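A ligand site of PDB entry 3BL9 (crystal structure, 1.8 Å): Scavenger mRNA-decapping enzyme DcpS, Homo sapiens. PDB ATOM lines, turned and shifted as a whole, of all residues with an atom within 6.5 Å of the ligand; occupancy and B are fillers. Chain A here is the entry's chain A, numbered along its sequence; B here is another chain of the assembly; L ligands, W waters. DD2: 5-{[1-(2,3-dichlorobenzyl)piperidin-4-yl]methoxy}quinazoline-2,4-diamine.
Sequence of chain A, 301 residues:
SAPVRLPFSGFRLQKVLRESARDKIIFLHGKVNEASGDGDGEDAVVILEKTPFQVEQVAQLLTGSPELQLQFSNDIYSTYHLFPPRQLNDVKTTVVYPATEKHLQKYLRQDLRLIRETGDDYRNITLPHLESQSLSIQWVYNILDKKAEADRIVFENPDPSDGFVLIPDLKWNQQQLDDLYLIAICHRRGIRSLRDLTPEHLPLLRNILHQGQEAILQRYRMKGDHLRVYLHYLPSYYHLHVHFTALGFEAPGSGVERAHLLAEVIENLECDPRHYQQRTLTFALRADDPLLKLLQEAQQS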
ATOM      1  N   ARG A  18     -24.266  -7.652 -22.089  1.00  0.00           N
ATOM      2  CA  ARG A  18     -25.249  -6.756 -21.512  1.00  0.00           C
ATOM      3  C   ARG A  18     -26.080  -6.110 -22.631  1.00  0.00           C
ATOM      4  O   ARG A  18     -25.589  -5.887 -23.730  1.00  0.00           O
ATOM      5  CB  ARG A  18     -24.498  -5.674 -20.723  1.00  0.00           C
ATOM      6  CG  ARG A  18     -25.334  -4.598 -20.079  1.00  0.00           C
ATOM      7  CD  ARG A  18     -24.454  -3.466 -19.572  1.00  0.00           C
ATOM      8  NE  ARG A  18     -23.490  -3.942 -18.592  1.00  0.00           N
ATOM      9  CZ  ARG A  18     -23.017  -3.227 -17.582  1.00  0.00           C
ATOM     10  NH1 ARG A  18     -23.409  -1.978 -17.384  1.00  0.00           N
ATOM     11  NH2 ARG A  18     -22.144  -3.788 -16.738  1.00  0.00           N
ATOM     12  N   PHE A  27     -23.808  -4.841 -25.617  1.00  0.00           N
ATOM     13  CA  PHE A  27     -22.396  -5.172 -25.394  1.00  0.00           C
ATOM     14  C   PHE A  27     -22.176  -6.654 -25.759  1.00  0.00           C
ATOM     15  O   PHE A  27     -22.787  -7.562 -25.147  1.00  0.00           O
ATOM     16  CB  PHE A  27     -22.027  -4.983 -23.914  1.00  0.00           C
ATOM     17  CG  PHE A  27     -22.136  -3.570 -23.406  1.00  0.00           C
ATOM     18  CD1 PHE A  27     -23.374  -2.952 -23.254  1.00  0.00           C
ATOM     19  CD2 PHE A  27     -20.990  -2.865 -23.000  1.00  0.00           C
ATOM     20  CE1 PHE A  27     -23.476  -1.651 -22.768  1.00  0.00           C
ATOM     21  CE2 PHE A  27     -21.083  -1.566 -22.491  1.00  0.00           C
ATOM     22  CZ  PHE A  27     -22.332  -0.960 -22.401  1.00  0.00           C
ATOM     23  N   ILE A  47     -19.422  -2.735 -28.711  1.00  0.00           N
ATOM     24  CA  ILE A  47     -20.531  -2.044 -28.074  1.00  0.00           C
ATOM     25  C   ILE A  47     -21.236  -1.210 -29.148  1.00  0.00           C
ATOM     26  O   ILE A  47     -20.588  -0.430 -29.848  1.00  0.00           O
ATOM     27  CB  ILE A  47     -20.054  -1.136 -26.908  1.00  0.00           C
ATOM     28  CG1 ILE A  47     -19.171  -1.910 -25.918  1.00  0.00           C
ATOM     29  CG2 ILE A  47     -21.272  -0.543 -26.178  1.00  0.00           C
ATOM     30  CD1 ILE A  47     -18.396  -1.022 -24.992  1.00  0.00           C
ATOM     31  N   LYS A 106     -16.244  -6.919 -16.622  1.00  0.00           N
ATOM     32  CA  LYS A 106     -16.628  -5.527 -16.373  1.00  0.00           C
ATOM     33  C   LYS A 106     -17.945  -5.149 -17.048  1.00  0.00           C
ATOM     34  O   LYS A 106     -18.798  -4.473 -16.465  1.00  0.00           O
ATOM     35  CB  LYS A 106     -15.482  -4.664 -16.886  1.00  0.00           C
ATOM     36  CG  LYS A 106     -15.570  -3.202 -16.786  1.00  0.00           C
ATOM     37  CD  LYS A 106     -14.192  -2.664 -17.231  1.00  0.00           C
ATOM     38  CE  LYS A 106     -14.166  -1.225 -17.609  1.00  0.00           C
ATOM     39  NZ  LYS A 106     -12.734  -0.822 -17.757  1.00  0.00           N
ATOM     40  N   TYR A 107     -18.106  -5.619 -18.286  1.00  0.00           N
ATOM     41  CA  TYR A 107     -19.257  -5.258 -19.099  1.00  0.00           C
ATOM     42  C   TYR A 107     -20.446  -6.212 -18.914  1.00  0.00           C
ATOM     43  O   TYR A 107     -21.542  -5.925 -19.381  1.00  0.00           O
ATOM     44  CB  TYR A 107     -18.851  -5.196 -20.581  1.00  0.00           C
ATOM     45  CG  TYR A 107     -17.866  -4.082 -20.900  1.00  0.00           C
ATOM     46  CD1 TYR A 107     -16.603  -4.352 -21.414  1.00  0.00           C
ATOM     47  CD2 TYR A 107     -18.221  -2.743 -20.716  1.00  0.00           C
ATOM     48  CE1 TYR A 107     -15.709  -3.318 -21.716  1.00  0.00           C
ATOM     49  CE2 TYR A 107     -17.345  -1.722 -21.016  1.00  0.00           C
ATOM     50  CZ  TYR A 107     -16.079  -2.017 -21.490  1.00  0.00           C
ATOM     51  OH  TYR A 107     -15.202  -0.982 -21.794  1.00  0.00           O
ATOM     52  N   TRP A 139      -4.339   4.428 -22.062  1.00  0.00           N
ATOM     53  CA  TRP A 139      -5.087   5.383 -22.870  1.00  0.00           C
ATOM     54  C   TRP A 139      -5.089   6.771 -22.282  1.00  0.00           C
ATOM     55  O   TRP A 139      -5.083   7.761 -23.030  1.00  0.00           O
ATOM     56  CB  TRP A 139      -6.534   4.904 -23.088  1.00  0.00           C
ATOM     57  CG  TRP A 139      -7.468   4.983 -21.932  1.00  0.00           C
ATOM     58  CD1 TRP A 139      -7.847   3.966 -21.121  1.00  0.00           C
ATOM     59  CD2 TRP A 139      -8.221   6.127 -21.519  1.00  0.00           C
ATOM     60  NE1 TRP A 139      -8.752   4.403 -20.186  1.00  0.00           N
ATOM     61  CE2 TRP A 139      -9.016   5.719 -20.418  1.00  0.00           C
ATOM     62  CE3 TRP A 139      -8.307   7.449 -21.955  1.00  0.00           C
ATOM     63  CZ2 TRP A 139      -9.869   6.586 -19.753  1.00  0.00           C
ATOM     64  CZ3 TRP A 139      -9.180   8.324 -21.269  1.00  0.00           C
ATOM     65  CH2 TRP A 139      -9.949   7.880 -20.202  1.00  0.00           C
ATOM     66  N   VAL A 140      -5.106   6.839 -20.957  1.00  0.00           N
ATOM     67  CA  VAL A 140      -5.073   8.135 -20.261  1.00  0.00           C
ATOM     68  C   VAL A 140      -3.712   8.824 -20.524  1.00  0.00           C
ATOM     69  O   VAL A 140      -3.644   9.982 -20.956  1.00  0.00           O
ATOM     70  CB  VAL A 140      -5.340   7.988 -18.745  1.00  0.00           C
ATOM     71  CG1 VAL A 140      -5.194   9.333 -18.019  1.00  0.00           C
ATOM     72  CG2 VAL A 140      -6.681   7.329 -18.502  1.00  0.00           C
ATOM     73  N   ILE A 143      -3.217  10.263 -23.980  1.00  0.00           N
ATOM     74  CA  ILE A 143      -3.795  11.598 -24.155  1.00  0.00           C
ATOM     75  C   ILE A 143      -2.871  12.667 -23.583  1.00  0.00           C
ATOM     76  O   ILE A 143      -2.601  13.658 -24.244  1.00  0.00           O
ATOM     77  CB  ILE A 143      -5.207  11.727 -23.527  1.00  0.00           C
ATOM     78  CG1 ILE A 143      -6.213  10.920 -24.330  1.00  0.00           C
ATOM     79  CG2 ILE A 143      -5.629  13.162 -23.512  1.00  0.00           C
ATOM     80  CD1 ILE A 143      -7.527  10.718 -23.628  1.00  0.00           C
ATOM     81  N   GLU A 149      -5.053  10.845 -29.844  1.00  0.00           N
ATOM     82  CA  GLU A 149      -6.094  11.892 -29.743  1.00  0.00           C
ATOM     83  C   GLU A 149      -5.593  13.341 -29.618  1.00  0.00           C
ATOM     84  O   GLU A 149      -6.364  14.215 -29.233  1.00  0.00           O
ATOM     85  CB  GLU A 149      -7.053  11.616 -28.560  1.00  0.00           C
ATOM     86  CG  GLU A 149      -7.687  10.242 -28.568  1.00  0.00           C
ATOM     87  CD  GLU A 149      -8.705  10.069 -27.465  1.00  0.00           C
ATOM     88  OE1 GLU A 149      -8.590   9.067 -26.714  1.00  0.00           O
ATOM     89  OE2 GLU A 149      -9.614  10.922 -27.325  1.00  0.00           O
ATOM     90  N   ARG A 152      -7.749  15.904 -31.071  1.00  0.00           N
ATOM     91  CA  ARG A 152      -9.108  16.024 -30.503  1.00  0.00           C
ATOM     92  C   ARG A 152      -9.208  16.934 -29.262  1.00  0.00           C
ATOM     93  O   ARG A 152     -10.305  17.221 -28.785  1.00  0.00           O
ATOM     94  CB  ARG A 152      -9.653  14.645 -30.089  1.00  0.00           C
ATOM     95  CG  ARG A 152      -9.647  13.566 -31.114  1.00  0.00           C
ATOM     96  CD  ARG A 152     -10.257  12.295 -30.518  1.00  0.00           C
ATOM     97  NE  ARG A 152     -11.702  12.448 -30.607  1.00  0.00           N
ATOM     98  CZ  ARG A 152     -12.573  12.478 -29.613  1.00  0.00           C
ATOM     99  NH1 ARG A 152     -12.244  12.291 -28.353  1.00  0.00           N
ATOM    100  NH2 ARG A 152     -13.815  12.661 -29.921  1.00  0.00           N
ATOM    101  N   ILE A 167     -11.000  17.153 -23.185  1.00  0.00           N
ATOM    102  CA  ILE A 167     -11.160  16.378 -24.420  1.00  0.00           C
ATOM    103  C   ILE A 167     -12.550  15.736 -24.425  1.00  0.00           C
ATOM    104  O   ILE A 167     -13.034  15.329 -23.363  1.00  0.00           O
ATOM    105  CB  ILE A 167     -10.003  15.351 -24.576  1.00  0.00           C
ATOM    106  CG1 ILE A 167     -10.014  14.669 -25.936  1.00  0.00           C
ATOM    107  CG2 ILE A 167     -10.002  14.287 -23.400  1.00  0.00           C
ATOM    108  CD1 ILE A 167      -8.785  13.736 -26.160  1.00  0.00           C
ATOM    109  N   PRO A 168     -13.216  15.688 -25.610  1.00  0.00           N
ATOM    110  CA  PRO A 168     -14.508  15.002 -25.621  1.00  0.00           C
ATOM    111  C   PRO A 168     -14.375  13.549 -25.149  1.00  0.00           C
ATOM    112  O   PRO A 168     -13.396  12.856 -25.496  1.00  0.00           O
ATOM    113  CB  PRO A 168     -14.919  15.059 -27.106  1.00  0.00           C
ATOM    114  CG  PRO A 168     -14.159  16.272 -27.654  1.00  0.00           C
ATOM    115  CD  PRO A 168     -12.854  16.231 -26.934  1.00  0.00           C
ATOM    116  N   ASP A 169     -15.315  13.098 -24.334  1.00  0.00           N
ATOM    117  CA  ASP A 169     -15.253  11.739 -23.835  1.00  0.00           C
ATOM    118  C   ASP A 169     -15.636  10.778 -24.965  1.00  0.00           C
ATOM    119  O   ASP A 169     -16.419  11.149 -25.852  1.00  0.00           O
ATOM    120  CB  ASP A 169     -16.187  11.582 -22.647  1.00  0.00           C
ATOM    121  CG  ASP A 169     -16.061  10.258 -21.989  1.00  0.00           C
ATOM    122  OD1 ASP A 169     -16.864   9.361 -22.317  1.00  0.00           O
ATOM    123  OD2 ASP A 169     -15.139  10.087 -21.177  1.00  0.00           O
ATOM    124  N   LEU A 170     -15.079   9.565 -24.898  1.00  0.00           N
ATOM    125  CA  LEU A 170     -15.376   8.470 -25.814  1.00  0.00           C
ATOM    126  C   LEU A 170     -16.866   8.286 -26.027  1.00  0.00           C
ATOM    127  O   LEU A 170     -17.288   7.978 -27.130  1.00  0.00           O
ATOM    128  CB  LEU A 170     -14.839   7.154 -25.248  1.00  0.00           C
ATOM    129  CG  LEU A 170     -15.134   5.806 -25.939  1.00  0.00           C
ATOM    130  CD1 LEU A 170     -14.428   5.755 -27.245  1.00  0.00           C
ATOM    131  CD2 LEU A 170     -14.670   4.664 -25.041  1.00  0.00           C
ATOM    132  N   LYS A 171     -17.655   8.463 -24.959  1.00  0.00           N
ATOM    133  CA  LYS A 171     -19.120   8.330 -25.014  1.00  0.00           C
ATOM    134  C   LYS A 171     -19.797   9.273 -26.005  1.00  0.00           C
ATOM    135  O   LYS A 171     -20.853   8.924 -26.561  1.00  0.00           O
ATOM    136  CB  LYS A 171     -19.718   8.552 -23.604  1.00  0.00           C
ATOM    137  CG  LYS A 171     -21.261   8.520 -23.458  1.00  0.00           C
ATOM    138  CD  LYS A 171     -21.812   7.122 -23.592  1.00  0.00           C
ATOM    139  CE  LYS A 171     -23.260   7.017 -23.204  1.00  0.00           C
ATOM    140  NZ  LYS A 171     -23.631   5.576 -23.241  1.00  0.00           N
ATOM    141  N   TYR A 181     -20.419  16.096 -23.585  1.00  0.00           N
ATOM    142  CA  TYR A 181     -19.701  15.332 -22.567  1.00  0.00           C
ATOM    143  C   TYR A 181     -18.201  15.361 -22.864  1.00  0.00           C
ATOM    144  O   TYR A 181     -17.696  14.689 -23.781  1.00  0.00           O
ATOM    145  CB  TYR A 181     -20.257  13.919 -22.502  1.00  0.00           C
ATOM    146  CG  TYR A 181     -19.659  12.985 -21.474  1.00  0.00           C
ATOM    147  CD1 TYR A 181     -19.947  11.624 -21.507  1.00  0.00           C
ATOM    148  CD2 TYR A 181     -18.787  13.468 -20.476  1.00  0.00           C
ATOM    149  CE1 TYR A 181     -19.386  10.764 -20.555  1.00  0.00           C
ATOM    150  CE2 TYR A 181     -18.248  12.627 -19.536  1.00  0.00           C
ATOM    151  CZ  TYR A 181     -18.542  11.295 -19.572  1.00  0.00           C
ATOM    152  OH  TYR A 181     -17.980  10.485 -18.624  1.00  0.00           O
ATOM    153  N   ILE A 183     -14.240  15.281 -20.789  1.00  0.00           N
ATOM    154  CA  ILE A 183     -13.503  14.998 -19.556  1.00  0.00           C
ATOM    155  C   ILE A 183     -12.272  15.890 -19.494  1.00  0.00           C
ATOM    156  O   ILE A 183     -11.666  16.174 -20.525  1.00  0.00           O
ATOM    157  CB  ILE A 183     -13.117  13.502 -19.398  1.00  0.00           C
ATOM    158  CG1 ILE A 183     -12.452  12.952 -20.665  1.00  0.00           C
ATOM    159  CG2 ILE A 183     -14.364  12.664 -19.029  1.00  0.00           C
ATOM    160  CD1 ILE A 183     -11.902  11.529 -20.511  1.00  0.00           C
ATOM    161  N   ILE A 185      -8.688  15.673 -17.772  1.00  0.00           N
ATOM    162  CA  ILE A 185      -7.730  14.756 -17.180  1.00  0.00           C
ATOM    163  C   ILE A 185      -6.530  15.569 -16.667  1.00  0.00           C
ATOM    164  O   ILE A 185      -5.867  16.240 -17.467  1.00  0.00           O
ATOM    165  CB  ILE A 185      -7.246  13.730 -18.223  1.00  0.00           C
ATOM    166  CG1 ILE A 185      -8.452  12.988 -18.838  1.00  0.00           C
ATOM    167  CG2 ILE A 185      -6.252  12.739 -17.598  1.00  0.00           C
ATOM    168  CD1 ILE A 185      -8.069  12.134 -20.052  1.00  0.00           C
ATOM    169  N   SER A 236     -14.215   4.897 -12.679  1.00  0.00           N
ATOM    170  CA  SER A 236     -13.989   3.741 -13.544  1.00  0.00           C
ATOM    171  C   SER A 236     -12.532   3.525 -13.844  1.00  0.00           C
ATOM    172  O   SER A 236     -12.143   2.431 -14.272  1.00  0.00           O
ATOM    173  CB  SER A 236     -14.763   3.865 -14.836  1.00  0.00           C
ATOM    174  OG  SER A 236     -16.158   3.768 -14.615  1.00  0.00           O
ATOM    175  N   TYR A 237     -11.730   4.576 -13.659  1.00  0.00           N
ATOM    176  CA  TYR A 237     -10.283   4.497 -13.794  1.00  0.00           C
ATOM    177  C   TYR A 237      -9.644   5.434 -12.786  1.00  0.00           C
ATOM    178  O   TYR A 237     -10.172   6.513 -12.536  1.00  0.00           O
ATOM    179  CB  TYR A 237      -9.820   4.796 -15.229  1.00  0.00           C
ATOM    180  CG  TYR A 237     -10.464   6.002 -15.894  1.00  0.00           C
ATOM    181  CD1 TYR A 237      -9.804   7.221 -15.988  1.00  0.00           C
ATOM    182  CD2 TYR A 237     -11.712   5.920 -16.460  1.00  0.00           C
ATOM    183  CE1 TYR A 237     -10.389   8.324 -16.617  1.00  0.00           C
ATOM    184  CE2 TYR A 237     -12.311   7.028 -17.075  1.00  0.00           C
ATOM    185  CZ  TYR A 237     -11.642   8.210 -17.146  1.00  0.00           C
ATOM    186  OH  TYR A 237     -12.262   9.276 -17.780  1.00  0.00           O
ATOM    187  N   ARG A 258     -23.075   8.341  -7.079  1.00  0.00           N
ATOM    188  CA  ARG A 258     -21.754   8.307  -7.727  1.00  0.00           C
ATOM    189  C   ARG A 258     -21.113   9.664  -7.947  1.00  0.00           C
ATOM    190  O   ARG A 258     -19.878   9.782  -7.971  1.00  0.00           O
ATOM    191  CB  ARG A 258     -21.836   7.586  -9.080  1.00  0.00           C
ATOM    192  CG  ARG A 258     -20.458   7.159  -9.599  1.00  0.00           C
ATOM    193  CD  ARG A 258     -20.514   6.129 -10.642  1.00  0.00           C
ATOM    194  NE  ARG A 258     -19.169   5.682 -10.958  1.00  0.00           N
ATOM    195  CZ  ARG A 258     -18.740   5.321 -12.161  1.00  0.00           C
ATOM    196  NH1 ARG A 258     -19.546   5.339 -13.217  1.00  0.00           N
ATOM    197  NH2 ARG A 258     -17.485   4.959 -12.324  1.00  0.00           N
ATOM    198  N   ARG A 286     -20.654  -3.689  -7.660  1.00  0.00           N
ATOM    199  CA  ARG A 286     -21.257  -4.877  -8.272  1.00  0.00           C
ATOM    200  C   ARG A 286     -21.272  -5.992  -7.231  1.00  0.00           C
ATOM    201  O   ARG A 286     -20.334  -6.126  -6.460  1.00  0.00           O
ATOM    202  CB  ARG A 286     -20.447  -5.360  -9.473  1.00  0.00           C
ATOM    203  CG  ARG A 286     -20.287  -4.355 -10.579  1.00  0.00           C
ATOM    204  CD  ARG A 286     -19.102  -4.730 -11.463  1.00  0.00           C
ATOM    205  NE  ARG A 286     -19.174  -6.105 -11.955  1.00  0.00           N
ATOM    206  CZ  ARG A 286     -19.761  -6.472 -13.102  1.00  0.00           C
ATOM    207  NH1 ARG A 286     -20.345  -5.592 -13.886  1.00  0.00           N
ATOM    208  NH2 ARG A 286     -19.755  -7.756 -13.443  1.00  0.00           N
ATOM    209  N   PHE B  72     -12.186   7.803 -33.863  1.00  0.00           N
ATOM    210  CA  PHE B  72     -10.776   7.815 -33.418  1.00  0.00           C
ATOM    211  C   PHE B  72     -10.389   6.489 -32.747  1.00  0.00           C
ATOM    212  O   PHE B  72     -11.258   5.674 -32.434  1.00  0.00           O
ATOM    213  CB  PHE B  72     -10.516   8.976 -32.420  1.00  0.00           C
ATOM    214  CG  PHE B  72     -11.149   8.795 -31.060  1.00  0.00           C
ATOM    215  CD1 PHE B  72     -10.442   8.186 -30.026  1.00  0.00           C
ATOM    216  CD2 PHE B  72     -12.452   9.231 -30.814  1.00  0.00           C
ATOM    217  CE1 PHE B  72     -11.014   8.024 -28.757  1.00  0.00           C
ATOM    218  CE2 PHE B  72     -13.035   9.078 -29.544  1.00  0.00           C
ATOM    219  CZ  PHE B  72     -12.322   8.452 -28.513  1.00  0.00           C
ATOM    220  N   SER B  73      -9.092   6.277 -32.519  1.00  0.00           N
ATOM    221  CA  SER B  73      -8.609   5.155 -31.694  1.00  0.00           C
ATOM    222  C   SER B  73      -7.541   5.608 -30.688  1.00  0.00           C
ATOM    223  O   SER B  73      -6.928   6.679 -30.853  1.00  0.00           O
ATOM    224  CB  SER B  73      -8.033   4.054 -32.568  1.00  0.00           C
ATOM    225  OG  SER B  73      -6.890   4.517 -33.271  1.00  0.00           O
ATOM    226  N   ASN B  74      -7.304   4.754 -29.697  1.00  0.00           N
ATOM    227  CA  ASN B  74      -6.358   5.032 -28.609  1.00  0.00           C
ATOM    228  C   ASN B  74      -6.098   3.721 -27.890  1.00  0.00           C
ATOM    229  O   ASN B  74      -6.984   3.169 -27.213  1.00  0.00           O
ATOM    230  CB  ASN B  74      -6.935   6.079 -27.674  1.00  0.00           C
ATOM    231  CG  ASN B  74      -6.010   6.420 -26.488  1.00  0.00           C
ATOM    232  OD1 ASN B  74      -5.086   5.677 -26.206  1.00  0.00           O
ATOM    233  ND2 ASN B  74      -6.286   7.525 -25.807  1.00  0.00           N
ATOM    234  N   ASP B  75      -4.915   3.173 -28.063  1.00  0.00           N
ATOM    235  CA  ASP B  75      -4.556   1.931 -27.392  1.00  0.00           C
ATOM    236  C   ASP B  75      -5.558   0.859 -27.893  1.00  0.00           C
ATOM    237  O   ASP B  75      -5.778   0.783 -29.123  1.00  0.00           O
ATOM    238  CB  ASP B  75      -4.528   2.138 -25.866  1.00  0.00           C
ATOM    239  CG  ASP B  75      -3.915   0.993 -25.112  1.00  0.00           C
ATOM    240  OD1 ASP B  75      -2.700   0.736 -25.279  1.00  0.00           O
ATOM    241  OD2 ASP B  75      -4.624   0.368 -24.314  1.00  0.00           O
ATOM    242  N   TYR B  77      -8.742   0.733 -27.668  1.00  0.00           N
ATOM    243  CA  TYR B  77     -10.097   1.314 -27.892  1.00  0.00           C
ATOM    244  C   TYR B  77     -10.215   2.012 -29.221  1.00  0.00           C
ATOM    245  O   TYR B  77      -9.321   2.746 -29.664  1.00  0.00           O
ATOM    246  CB  TYR B  77     -10.439   2.333 -26.829  1.00  0.00           C
ATOM    247  CG  TYR B  77     -10.524   1.762 -25.438  1.00  0.00           C
ATOM    248  CD1 TYR B  77      -9.405   1.709 -24.602  1.00  0.00           C
ATOM    249  CD2 TYR B  77     -11.733   1.302 -24.937  1.00  0.00           C
ATOM    250  CE1 TYR B  77      -9.496   1.209 -23.313  1.00  0.00           C
ATOM    251  CE2 TYR B  77     -11.828   0.783 -23.660  1.00  0.00           C
ATOM    252  CZ  TYR B  77     -10.705   0.725 -22.861  1.00  0.00           C
ATOM    253  OH  TYR B  77     -10.812   0.204 -21.592  1.00  0.00           O
HETATM  254  C1  DD2 L   1     -18.813   1.134 -18.538  1.00  0.00           C
HETATM  255  C2  DD2 L   1     -17.607   1.603 -17.848  1.00  0.00           C
HETATM  256  C3  DD2 L   1     -17.048   0.777 -16.881  1.00  0.00           C
HETATM  257  C4  DD2 L   1     -17.577  -0.476 -16.599  1.00  0.00           C
HETATM  258  C5  DD2 L   1     -18.700  -0.964 -17.249  1.00  0.00           C
HETATM  259  C6  DD2 L   1     -19.320  -0.199 -18.205  1.00  0.00           C
HETATM  260  C9  DD2 L   1     -17.090   2.987 -18.163  1.00  0.00           C
HETATM  261  C11 DD2 L   1     -16.089   4.227 -20.007  1.00  0.00           C
HETATM  262  C14 DD2 L   1     -13.748   2.426 -19.983  1.00  0.00           C
HETATM  263  C15 DD2 L   1     -14.905   2.102 -19.021  1.00  0.00           C
HETATM  264  O17 DD2 L   1     -12.413   5.400 -21.838  1.00  0.00           O
HETATM  265  C18 DD2 L   1     -11.557   5.694 -22.868  1.00  0.00           C
HETATM  266  C19 DD2 L   1     -10.695   4.748 -23.410  1.00  0.00           C
HETATM  267  C20 DD2 L   1      -9.808   5.099 -24.448  1.00  0.00           C
HETATM  268  C21 DD2 L   1      -9.769   6.369 -24.975  1.00  0.00           C
HETATM  269  C22 DD2 L   1     -10.593   7.361 -24.514  1.00  0.00           C
HETATM  270  C24 DD2 L   1     -12.395   8.162 -22.905  1.00  0.00           C
HETATM  271  C26 DD2 L   1     -11.411   9.540 -24.564  1.00  0.00           C
HETATM  272 CL8  DD2 L   1     -19.599   2.097 -19.820  1.00  0.00          CL
HETATM  273 CL7  DD2 L   1     -20.764  -0.751 -19.068  1.00  0.00          CL
HETATM  274  N10 DD2 L   1     -16.001   3.055 -19.119  1.00  0.00           N
HETATM  275  C13 DD2 L   1     -13.616   3.894 -20.374  1.00  0.00           C
HETATM  276  C12 DD2 L   1     -14.926   4.341 -20.998  1.00  0.00           C
HETATM  277  C16 DD2 L   1     -12.538   4.039 -21.439  1.00  0.00           C
HETATM  278  C23 DD2 L   1     -11.539   7.058 -23.408  1.00  0.00           C
HETATM  279  N29 DD2 L   1     -13.297   8.000 -21.911  1.00  0.00           N
HETATM  280  N25 DD2 L   1     -12.300   9.344 -23.532  1.00  0.00           N
HETATM  281  N28 DD2 L   1     -11.348  10.759 -25.107  1.00  0.00           N
HETATM  282  N27 DD2 L   1     -10.563   8.593 -25.021  1.00  0.00           N
HETATM  283  O   HOH W   1     -12.318   2.193 -17.104  1.00  0.00           O
HETATM  284  O   HOH W   2     -12.998  -0.939 -20.393  1.00  0.00           O
HETATM  285  O   HOH W   3     -16.841   7.022 -20.977  1.00  0.00           O
HETATM  286  O   HOH W   4     -18.366   5.019 -16.028  1.00  0.00           O
HETATM  287  O   HOH W   5     -14.460   8.990 -18.787  1.00  0.00           O
HETATM  288  O   HOH W   6     -16.264   1.547 -21.792  1.00  0.00           O
HETATM  289  O   HOH W   7     -18.913  -2.594 -14.237  1.00  0.00           O
HETATM  290  O   HOH W   8     -16.505   1.278 -13.586  1.00  0.00           O
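Arg 18 touches the ligand (NH1 to CL7, 3.4 Å).
CE2 of Phe 27 touches CL7 of the ligand, at 3.5 Å.
CG of Lys 106 touches C4 of the ligand, 3.4 Å away.
CD2 of Tyr 107 touches CL7 of the ligand (3.6 Å).
Trp 139 touches the ligand (CD2 to C19, 3.4 Å).
Ile 143 touches the ligand.
Arg 152 touches the ligand (NH1 to N28, 3.7 Å).
Ile 183 touches the ligand (CD1 to N25, 3.7 Å).
Ser 236 touches the ligand (OG to C9, 3.8 Å).
Phe 72 of chain B touches the ligand.
Asn 74 of chain B touches the ligand.
Tyr 77 of chain B touches the ligand.
Hydrophobic or aromatic side chains that line the ligand: Phe 27, Tyr 107, Trp 139, Ile 143, Leu 170, Ile 183, Phe 72 of chain B and Tyr 77 of chain B.
Of the 27 residues printed, 16 come within 4 Å of the ligand.
The nearest printed residue that does not touch the ligand is Ile 167 (4.1 Å).
Water W4 lies within hydrogen-bond range of OG of Ser 236 and NH1 of Arg 258.
Water W1 lies within hydrogen-bond range of the backbone carbonyl oxygen of Ser 236 (2.8 Å) and the side-chain amino group of Lys 106 (3.1 Å).
Water W7 bridges the backbone carbonyl oxygen (O) of Lys 106 (2.9 Å) and the guanidinium group (NH1) of Arg 286 (3.3 Å).
Water W2 lies within hydrogen-bond range of OH of Tyr 107 (2.6 Å), NZ of Lys 106 (2.7 Å) and OH of Tyr 77 of chain B (2.7 Å).
Water W5 lies within hydrogen-bond range of the side-chain hydroxyl (OH) of Tyr 237, the side-chain carboxylate (OD2) of Asp 169 and a nitrogen (N29) of the ligand.
OE1 of Glu 149 is in hydrogen-bond range of N27 of the ligand, at 2.6 Å.
A nitrogen (N29) of the ligand sits at hydrogen-bond distance from the side-chain carboxylate (OD2) of Asp 169.
N28 of the ligand sits at hydrogen-bond distance from O of Pro 168 (3.0 Å).
A nitrogen (N25) of the ligand lies within hydrogen-bond range of the backbone NH of Leu 170, 3.1 Å away.
The guanidinium group of Arg 152 lies within salt-bridge range of the side-chain carboxylate of Glu 149 (3.1 Å).
ND2 of Asn 74 of chain B sits at hydrogen-bond distance from OE1 of Glu 149, 2.9 Å away.
N of Asp 169 is in hydrogen-bond range of O of Tyr 181.
The guanidinium group (NH1) of Arg 152 sits at hydrogen-bond distance from the backbone carbonyl oxygen (O) of Pro 168 (3.1 Å).
O of Arg 18 is in hydrogen-bond range of N of Phe 27 (2.8 Å).
The backbone carbonyl oxygen (O) of Tyr 107 is in hydrogen-bond range of the guanidinium group (NE) of Arg 18 (2.9 Å).
The backbone carbonyl oxygen (O) of Trp 139 sits at hydrogen-bond distance from the side-chain amide nitrogen (ND2) of Asn 74 of chain B (3.0 Å).
The side-chain hydroxyl of Ser 236 is in hydrogen-bond range of the guanidinium group of Arg 258, at 2.9 Å.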
